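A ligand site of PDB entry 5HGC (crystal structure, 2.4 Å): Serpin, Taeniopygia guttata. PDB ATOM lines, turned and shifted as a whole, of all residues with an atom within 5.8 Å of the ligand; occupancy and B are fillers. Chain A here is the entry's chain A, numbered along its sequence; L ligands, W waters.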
ATOM      1  N   VAL A  12     -20.128  -2.441  -8.824  1.00  0.00           N
ATOM      2  CA  VAL A  12     -20.374  -3.348  -9.961  1.00  0.00           C
ATOM      3  C   VAL A  12     -19.085  -3.792 -10.677  1.00  0.00           C
ATOM      4  O   VAL A  12     -18.920  -5.002 -10.960  1.00  0.00           O
ATOM      5  CB  VAL A  12     -21.461  -2.765 -10.888  1.00  0.00           C
ATOM      6  CG1 VAL A  12     -21.478  -3.501 -12.187  1.00  0.00           C
ATOM      7  CG2 VAL A  12     -22.845  -2.836 -10.233  1.00  0.00           C
ATOM      8  N   PRO A  13     -18.150  -2.861 -10.937  1.00  0.00           N
ATOM      9  CA  PRO A  13     -16.937  -3.384 -11.604  1.00  0.00           C
ATOM     10  C   PRO A  13     -16.043  -4.203 -10.674  1.00  0.00           C
ATOM     11  O   PRO A  13     -15.456  -5.229 -11.079  1.00  0.00           O
ATOM     12  CB  PRO A  13     -16.202  -2.137 -12.095  1.00  0.00           C
ATOM     13  CG  PRO A  13     -17.064  -0.974 -11.744  1.00  0.00           C
ATOM     14  CD  PRO A  13     -18.139  -1.397 -10.791  1.00  0.00           C
ATOM     15  N   ALA A  16     -17.390  -7.710 -10.179  1.00  0.00           N
ATOM     16  CA  ALA A  16     -17.196  -8.507 -11.408  1.00  0.00           C
ATOM     17  C   ALA A  16     -15.770  -8.927 -11.597  1.00  0.00           C
ATOM     18  O   ALA A  16     -15.501 -10.091 -11.872  1.00  0.00           O
ATOM     19  CB  ALA A  16     -17.727  -7.786 -12.635  1.00  0.00           C
ATOM     20  N   ARG A 226     -28.724 -16.132 -23.996  1.00  0.00           N
ATOM     21  CA  ARG A 226     -29.158 -15.529 -22.755  1.00  0.00           C
ATOM     22  C   ARG A 226     -30.667 -15.670 -22.534  1.00  0.00           C
ATOM     23  O   ARG A 226     -31.459 -15.293 -23.382  1.00  0.00           O
ATOM     24  CB  ARG A 226     -28.736 -14.060 -22.715  1.00  0.00           C
ATOM     25  CG  ARG A 226     -29.144 -13.374 -21.434  1.00  0.00           C
ATOM     26  CD  ARG A 226     -30.479 -12.686 -21.646  1.00  0.00           C
ATOM     27  NE  ARG A 226     -30.226 -11.363 -22.219  1.00  0.00           N
ATOM     28  CZ  ARG A 226     -29.637 -10.374 -21.561  1.00  0.00           C
ATOM     29  NH1 ARG A 226     -29.261 -10.540 -20.269  1.00  0.00           N
ATOM     30  NH2 ARG A 226     -29.404  -9.239 -22.171  1.00  0.00           N
ATOM     31  N   HIS A 228     -33.889 -15.036 -19.769  1.00  0.00           N
ATOM     32  CA  HIS A 228     -34.289 -14.320 -18.557  1.00  0.00           C
ATOM     33  C   HIS A 228     -35.005 -15.237 -17.627  1.00  0.00           C
ATOM     34  O   HIS A 228     -35.790 -16.120 -18.038  1.00  0.00           O
ATOM     35  CB  HIS A 228     -35.174 -13.123 -18.850  1.00  0.00           C
ATOM     36  CG  HIS A 228     -34.463 -12.027 -19.571  1.00  0.00           C
ATOM     37  ND1 HIS A 228     -33.254 -11.518 -19.138  1.00  0.00           N
ATOM     38  CD2 HIS A 228     -34.792 -11.332 -20.677  1.00  0.00           C
ATOM     39  CE1 HIS A 228     -32.853 -10.566 -19.963  1.00  0.00           C
ATOM     40  NE2 HIS A 228     -33.780 -10.432 -20.895  1.00  0.00           N
ATOM     41  N   THR A 234     -30.917 -13.117 -14.705  1.00  0.00           N
ATOM     42  CA  THR A 234     -30.777 -13.554 -16.085  1.00  0.00           C
ATOM     43  C   THR A 234     -29.645 -14.589 -16.184  1.00  0.00           C
ATOM     44  O   THR A 234     -28.704 -14.541 -15.401  1.00  0.00           O
ATOM     45  CB  THR A 234     -30.520 -12.302 -16.988  1.00  0.00           C
ATOM     46  OG1 THR A 234     -30.696 -12.654 -18.361  1.00  0.00           O
ATOM     47  CG2 THR A 234     -29.120 -11.665 -16.729  1.00  0.00           C
ATOM     48  N   PHE A 236     -26.694 -16.320 -18.697  1.00  0.00           N
ATOM     49  CA  PHE A 236     -25.863 -16.451 -19.941  1.00  0.00           C
ATOM     50  C   PHE A 236     -25.328 -17.864 -20.049  1.00  0.00           C
ATOM     51  O   PHE A 236     -24.684 -18.343 -19.109  1.00  0.00           O
ATOM     52  CB  PHE A 236     -24.637 -15.541 -19.921  1.00  0.00           C
ATOM     53  CG  PHE A 236     -24.952 -14.076 -20.128  1.00  0.00           C
ATOM     54  CD1 PHE A 236     -25.852 -13.372 -19.244  1.00  0.00           C
ATOM     55  CD2 PHE A 236     -24.349 -13.368 -21.185  1.00  0.00           C
ATOM     56  CE1 PHE A 236     -26.135 -12.008 -19.420  1.00  0.00           C
ATOM     57  CE2 PHE A 236     -24.639 -11.996 -21.372  1.00  0.00           C
ATOM     58  CZ  PHE A 236     -25.509 -11.314 -20.490  1.00  0.00           C
ATOM     59  N   LYS A 254     -14.810  -9.319 -17.150  1.00  0.00           N
ATOM     60  CA  LYS A 254     -16.033  -8.556 -17.259  1.00  0.00           C
ATOM     61  C   LYS A 254     -16.186  -7.790 -18.563  1.00  0.00           C
ATOM     62  O   LYS A 254     -17.289  -7.368 -18.913  1.00  0.00           O
ATOM     63  CB  LYS A 254     -16.169  -7.617 -16.080  1.00  0.00           C
ATOM     64  CG  LYS A 254     -15.127  -6.531 -15.998  1.00  0.00           C
ATOM     65  CD  LYS A 254     -15.781  -5.296 -15.376  1.00  0.00           C
ATOM     66  CE  LYS A 254     -14.770  -4.515 -14.536  1.00  0.00           C
ATOM     67  NZ  LYS A 254     -13.410  -4.375 -15.134  1.00  0.00           N
ATOM     68  N   GLU A 255     -15.073  -7.595 -19.255  1.00  0.00           N
ATOM     69  CA  GLU A 255     -15.069  -6.925 -20.545  1.00  0.00           C
ATOM     70  C   GLU A 255     -15.664  -7.898 -21.578  1.00  0.00           C
ATOM     71  O   GLU A 255     -16.525  -7.463 -22.374  1.00  0.00           O
ATOM     72  CB  GLU A 255     -13.651  -6.481 -20.912  1.00  0.00           C
ATOM     73  CG  GLU A 255     -13.101  -5.257 -20.167  1.00  0.00           C
ATOM     74  CD  GLU A 255     -12.711  -5.461 -18.679  1.00  0.00           C
ATOM     75  OE1 GLU A 255     -12.237  -6.533 -18.188  1.00  0.00           O
ATOM     76  OE2 GLU A 255     -12.884  -4.455 -17.974  1.00  0.00           O
ATOM     77  N   ILE A 257     -17.871 -10.120 -20.856  1.00  0.00           N
ATOM     78  CA  ILE A 257     -19.304 -10.111 -20.531  1.00  0.00           C
ATOM     79  C   ILE A 257     -19.985  -8.913 -21.190  1.00  0.00           C
ATOM     80  O   ILE A 257     -21.032  -9.089 -21.797  1.00  0.00           O
ATOM     81  CB  ILE A 257     -19.620 -10.202 -19.003  1.00  0.00           C
ATOM     82  CG1 ILE A 257     -18.984 -11.454 -18.341  1.00  0.00           C
ATOM     83  CG2 ILE A 257     -21.113 -10.202 -18.798  1.00  0.00           C
ATOM     84  CD1 ILE A 257     -19.392 -12.784 -18.963  1.00  0.00           C
ATOM     85  N   GLN A 258     -19.385  -7.722 -21.064  1.00  0.00           N
ATOM     86  CA  GLN A 258     -19.961  -6.511 -21.606  1.00  0.00           C
ATOM     87  C   GLN A 258     -20.036  -6.535 -23.133  1.00  0.00           C
ATOM     88  O   GLN A 258     -21.026  -6.064 -23.703  1.00  0.00           O
ATOM     89  CB  GLN A 258     -19.176  -5.261 -21.176  1.00  0.00           C
ATOM     90  CG  GLN A 258     -19.842  -3.983 -21.694  1.00  0.00           C
ATOM     91  CD  GLN A 258     -19.799  -2.868 -20.684  1.00  0.00           C
ATOM     92  OE1 GLN A 258     -18.715  -2.516 -20.137  1.00  0.00           O
ATOM     93  NE2 GLN A 258     -20.981  -2.289 -20.411  1.00  0.00           N
ATOM     94  N   SER A 261     -23.111  -8.809 -23.929  1.00  0.00           N
ATOM     95  CA  SER A 261     -24.416  -8.249 -23.718  1.00  0.00           C
ATOM     96  C   SER A 261     -24.678  -7.045 -24.644  1.00  0.00           C
ATOM     97  O   SER A 261     -25.819  -6.805 -25.007  1.00  0.00           O
ATOM     98  CB  SER A 261     -24.642  -7.929 -22.255  1.00  0.00           C
ATOM     99  OG  SER A 261     -23.690  -6.976 -21.815  1.00  0.00           O
ATOM    100  N   LEU A 264     -25.843  -9.021 -28.016  1.00  0.00           N
ATOM    101  CA  LEU A 264     -26.938 -10.005 -28.098  1.00  0.00           C
ATOM    102  C   LEU A 264     -28.074  -9.461 -28.930  1.00  0.00           C
ATOM    103  O   LEU A 264     -28.341  -8.241 -28.856  1.00  0.00           O
ATOM    104  CB  LEU A 264     -27.509 -10.353 -26.723  1.00  0.00           C
ATOM    105  CG  LEU A 264     -26.543 -11.067 -25.811  1.00  0.00           C
ATOM    106  CD1 LEU A 264     -27.117 -10.887 -24.427  1.00  0.00           C
ATOM    107  CD2 LEU A 264     -26.339 -12.530 -26.192  1.00  0.00           C
ATOM    108  N   PHE A 360     -26.782 -13.640 -13.434  1.00  0.00           N
ATOM    109  CA  PHE A 360     -26.632 -12.256 -12.939  1.00  0.00           C
ATOM    110  C   PHE A 360     -27.977 -11.671 -12.454  1.00  0.00           C
ATOM    111  O   PHE A 360     -29.104 -12.142 -12.884  1.00  0.00           O
ATOM    112  CB  PHE A 360     -26.111 -11.310 -14.011  1.00  0.00           C
ATOM    113  CG  PHE A 360     -24.836 -11.761 -14.685  1.00  0.00           C
ATOM    114  CD1 PHE A 360     -24.884 -12.580 -15.846  1.00  0.00           C
ATOM    115  CD2 PHE A 360     -23.584 -11.352 -14.188  1.00  0.00           C
ATOM    116  CE1 PHE A 360     -23.722 -12.993 -16.477  1.00  0.00           C
ATOM    117  CE2 PHE A 360     -22.428 -11.765 -14.835  1.00  0.00           C
ATOM    118  CZ  PHE A 360     -22.502 -12.584 -15.981  1.00  0.00           C
ATOM    119  N   ASP A 361     -27.883 -10.647 -11.601  1.00  0.00           N
ATOM    120  CA  ASP A 361     -29.038  -9.785 -11.348  1.00  0.00           C
ATOM    121  C   ASP A 361     -28.992  -8.498 -12.206  1.00  0.00           C
ATOM    122  O   ASP A 361     -28.022  -7.743 -12.095  1.00  0.00           O
ATOM    123  CB  ASP A 361     -29.170  -9.478  -9.850  1.00  0.00           C
ATOM    124  CG  ASP A 361     -30.346  -8.541  -9.548  1.00  0.00           C
ATOM    125  OD1 ASP A 361     -31.382  -8.597 -10.274  1.00  0.00           O
ATOM    126  OD2 ASP A 361     -30.203  -7.717  -8.583  1.00  0.00           O
ATOM    127  N   ARG A 362     -30.042  -8.251 -13.013  1.00  0.00           N
ATOM    128  CA  ARG A 362     -30.169  -7.037 -13.850  1.00  0.00           C
ATOM    129  C   ARG A 362     -30.441  -5.737 -13.069  1.00  0.00           C
ATOM    130  O   ARG A 362     -30.017  -4.688 -13.530  1.00  0.00           O
ATOM    131  CB  ARG A 362     -31.192  -7.173 -14.976  1.00  0.00           C
ATOM    132  CG  ARG A 362     -30.849  -8.164 -16.066  1.00  0.00           C
ATOM    133  CD  ARG A 362     -32.110  -8.414 -16.895  1.00  0.00           C
ATOM    134  NE  ARG A 362     -32.958  -9.416 -16.250  1.00  0.00           N
ATOM    135  CZ  ARG A 362     -34.186  -9.764 -16.645  1.00  0.00           C
ATOM    136  NH1 ARG A 362     -34.714  -9.133 -17.710  1.00  0.00           N
ATOM    137  NH2 ARG A 362     -34.880 -10.715 -15.979  1.00  0.00           N
ATOM    138  N   ASN A 365     -26.764  -5.407 -11.315  1.00  0.00           N
ATOM    139  CA  ASN A 365     -25.633  -5.805 -12.143  1.00  0.00           C
ATOM    140  C   ASN A 365     -24.564  -6.580 -11.393  1.00  0.00           C
ATOM    141  O   ASN A 365     -23.391  -6.219 -11.453  1.00  0.00           O
ATOM    142  CB  ASN A 365     -25.009  -4.588 -12.810  1.00  0.00           C
ATOM    143  CG  ASN A 365     -25.899  -4.018 -13.924  1.00  0.00           C
ATOM    144  OD1 ASN A 365     -26.726  -4.715 -14.509  1.00  0.00           O
ATOM    145  ND2 ASN A 365     -25.733  -2.728 -14.183  1.00  0.00           N
ATOM    146  N   SER A 366     -24.979  -7.627 -10.692  1.00  0.00           N
ATOM    147  CA  SER A 366     -24.024  -8.456  -9.958  1.00  0.00           C
ATOM    148  C   SER A 366     -24.086  -9.876 -10.452  1.00  0.00           C
ATOM    149  O   SER A 366     -25.171 -10.374 -10.829  1.00  0.00           O
ATOM    150  CB  SER A 366     -24.246  -8.432  -8.442  1.00  0.00           C
ATOM    151  OG  SER A 366     -25.579  -8.782  -8.176  1.00  0.00           O
ATOM    152  N   THR A 367     -22.934 -10.532 -10.417  1.00  0.00           N
ATOM    153  CA  THR A 367     -22.832 -11.940 -10.710  1.00  0.00           C
ATOM    154  C   THR A 367     -23.260 -12.760  -9.505  1.00  0.00           C
ATOM    155  O   THR A 367     -22.613 -12.711  -8.442  1.00  0.00           O
ATOM    156  CB  THR A 367     -21.414 -12.312 -11.140  1.00  0.00           C
ATOM    157  OG1 THR A 367     -20.915 -11.271 -12.009  1.00  0.00           O
ATOM    158  CG2 THR A 367     -21.414 -13.674 -11.818  1.00  0.00           C
HETATM  159  C1  LIG L   1     -20.649  -4.370 -17.362  1.00  0.00           C
HETATM  160  C2  LIG L   1     -19.284  -3.809 -16.975  1.00  0.00           C
HETATM  161  C3  LIG L   1     -18.984  -4.022 -15.512  1.00  0.00           C
HETATM  162  C4  LIG L   1     -19.787  -4.963 -14.700  1.00  0.00           C
HETATM  163  C5  LIG L   1     -20.549  -5.882 -15.306  1.00  0.00           C
HETATM  164  C6  LIG L   1     -20.981  -7.109 -14.539  1.00  0.00           C
HETATM  165  C7  LIG L   1     -22.498  -7.354 -14.735  1.00  0.00           C
HETATM  166  C8  LIG L   1     -23.012  -7.203 -16.176  1.00  0.00           C
HETATM  167  C9  LIG L   1     -22.532  -5.865 -16.776  1.00  0.00           C
HETATM  168  C10 LIG L   1     -20.992  -5.728 -16.765  1.00  0.00           C
HETATM  169  C11 LIG L   1     -24.766  -5.684 -18.156  1.00  0.00           C
HETATM  170  C12 LIG L   1     -23.239  -5.453 -18.104  1.00  0.00           C
HETATM  171  C13 LIG L   1     -25.162  -7.075 -17.584  1.00  0.00           C
HETATM  172  C14 LIG L   1     -24.531  -7.208 -16.194  1.00  0.00           C
HETATM  173  C15 LIG L   1     -25.316  -8.302 -15.509  1.00  0.00           C
HETATM  174  C16 LIG L   1     -26.737  -8.167 -16.041  1.00  0.00           C
HETATM  175  C17 LIG L   1     -26.670  -7.192 -17.247  1.00  0.00           C
HETATM  176  C18 LIG L   1     -24.777  -8.260 -18.506  1.00  0.00           C
HETATM  177  C19 LIG L   1     -20.227  -6.828 -17.539  1.00  0.00           C
HETATM  178  C20 LIG L   1     -27.568  -7.616 -18.391  1.00  0.00           C
HETATM  179  C21 LIG L   1     -28.250  -6.581 -19.263  1.00  0.00           C
HETATM  180  O1  LIG L   1     -18.028  -3.452 -15.019  1.00  0.00           O
HETATM  181  O2  LIG L   1     -22.612  -6.273 -19.093  1.00  0.00           O
HETATM  182  O3  LIG L   1     -27.219  -5.921 -16.860  1.00  0.00           O
HETATM  183  O4  LIG L   1     -27.763  -8.800 -18.639  1.00  0.00           O
HETATM  184  O5  LIG L   1     -28.173  -7.143 -20.568  1.00  0.00           O
HETATM  185  O   HOH W   1     -28.324  -7.093 -24.053  1.00  0.00           O
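The side-chain amide oxygen of Asn 365 lies within hydrogen-bond range of an oxygen (O3) of the ligand (2.7 Å). An oxygen (O4) of the ligand is in hydrogen-bond range of the guanidinium group (NH1) of Arg 226. The side-chain hydroxyl (OG) of Ser 261 sits at hydrogen-bond distance from an oxygen (O2) of the ligand, 3.0 Å away.
O of Arg 362 sits close to OD1 of Asn 365, 3.4 Å away. The side-chain hydroxyl (OG1) of Thr 234 sits at hydrogen-bond distance from the guanidinium group (NH1) of Arg 226. OE2 of Glu 255 lies within salt-bridge range of NZ of Lys 254 (2.9 Å). The side-chain hydroxyl (OG) of Ser 261 sits at hydrogen-bond distance from the backbone carbonyl oxygen (O) of Gln 258, 3.4 Å away. The side-chain hydroxyl (OG) of Ser 261 is in hydrogen-bond range of the backbone carbonyl oxygen (O) of Ile 257, at 3.4 Å. N of Thr 234 lies within hydrogen-bond range of O of Phe 360, 2.7 Å away. The side-chain hydroxyl (OG1) of Thr 234 lies within hydrogen-bond range of a ring nitrogen (ND1) of His 228 (2.9 Å).
Val 12 touches the ligand. Pro 13 touches the ligand (CA to O1, 3.6 Å). CB of Ala 16 touches C6 of the ligand, 3.8 Å away. Thr 234 touches the ligand. CE1 of Phe 236 touches O4 of the ligand, 3.7 Å away. Lys 254 touches the ligand. Ile 257 touches the ligand. Gln 258 touches the ligand. CB of Phe 360 touches C15 of the ligand, 3.5 Å away. Hydrophobic or aromatic side chains that line the ligand: Val 12, Pro 13, Ala 16, Phe 236, Ile 257 and Phe 360. Within 4 Å of the ligand: Val 12, Pro 13, Ala 16, Arg 226, Thr 234, Phe 236, Lys 254, Ile 257, Gln 258, Ser 261, Phe 360 and Asn 365.
Water W1 lies within hydrogen-bond range of the backbone carbonyl oxygen of Ser 261 (2.7 Å), the guanidinium group of Arg 226 (3.1 Å) and an oxygen (O5) of the ligand (3.5 Å).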
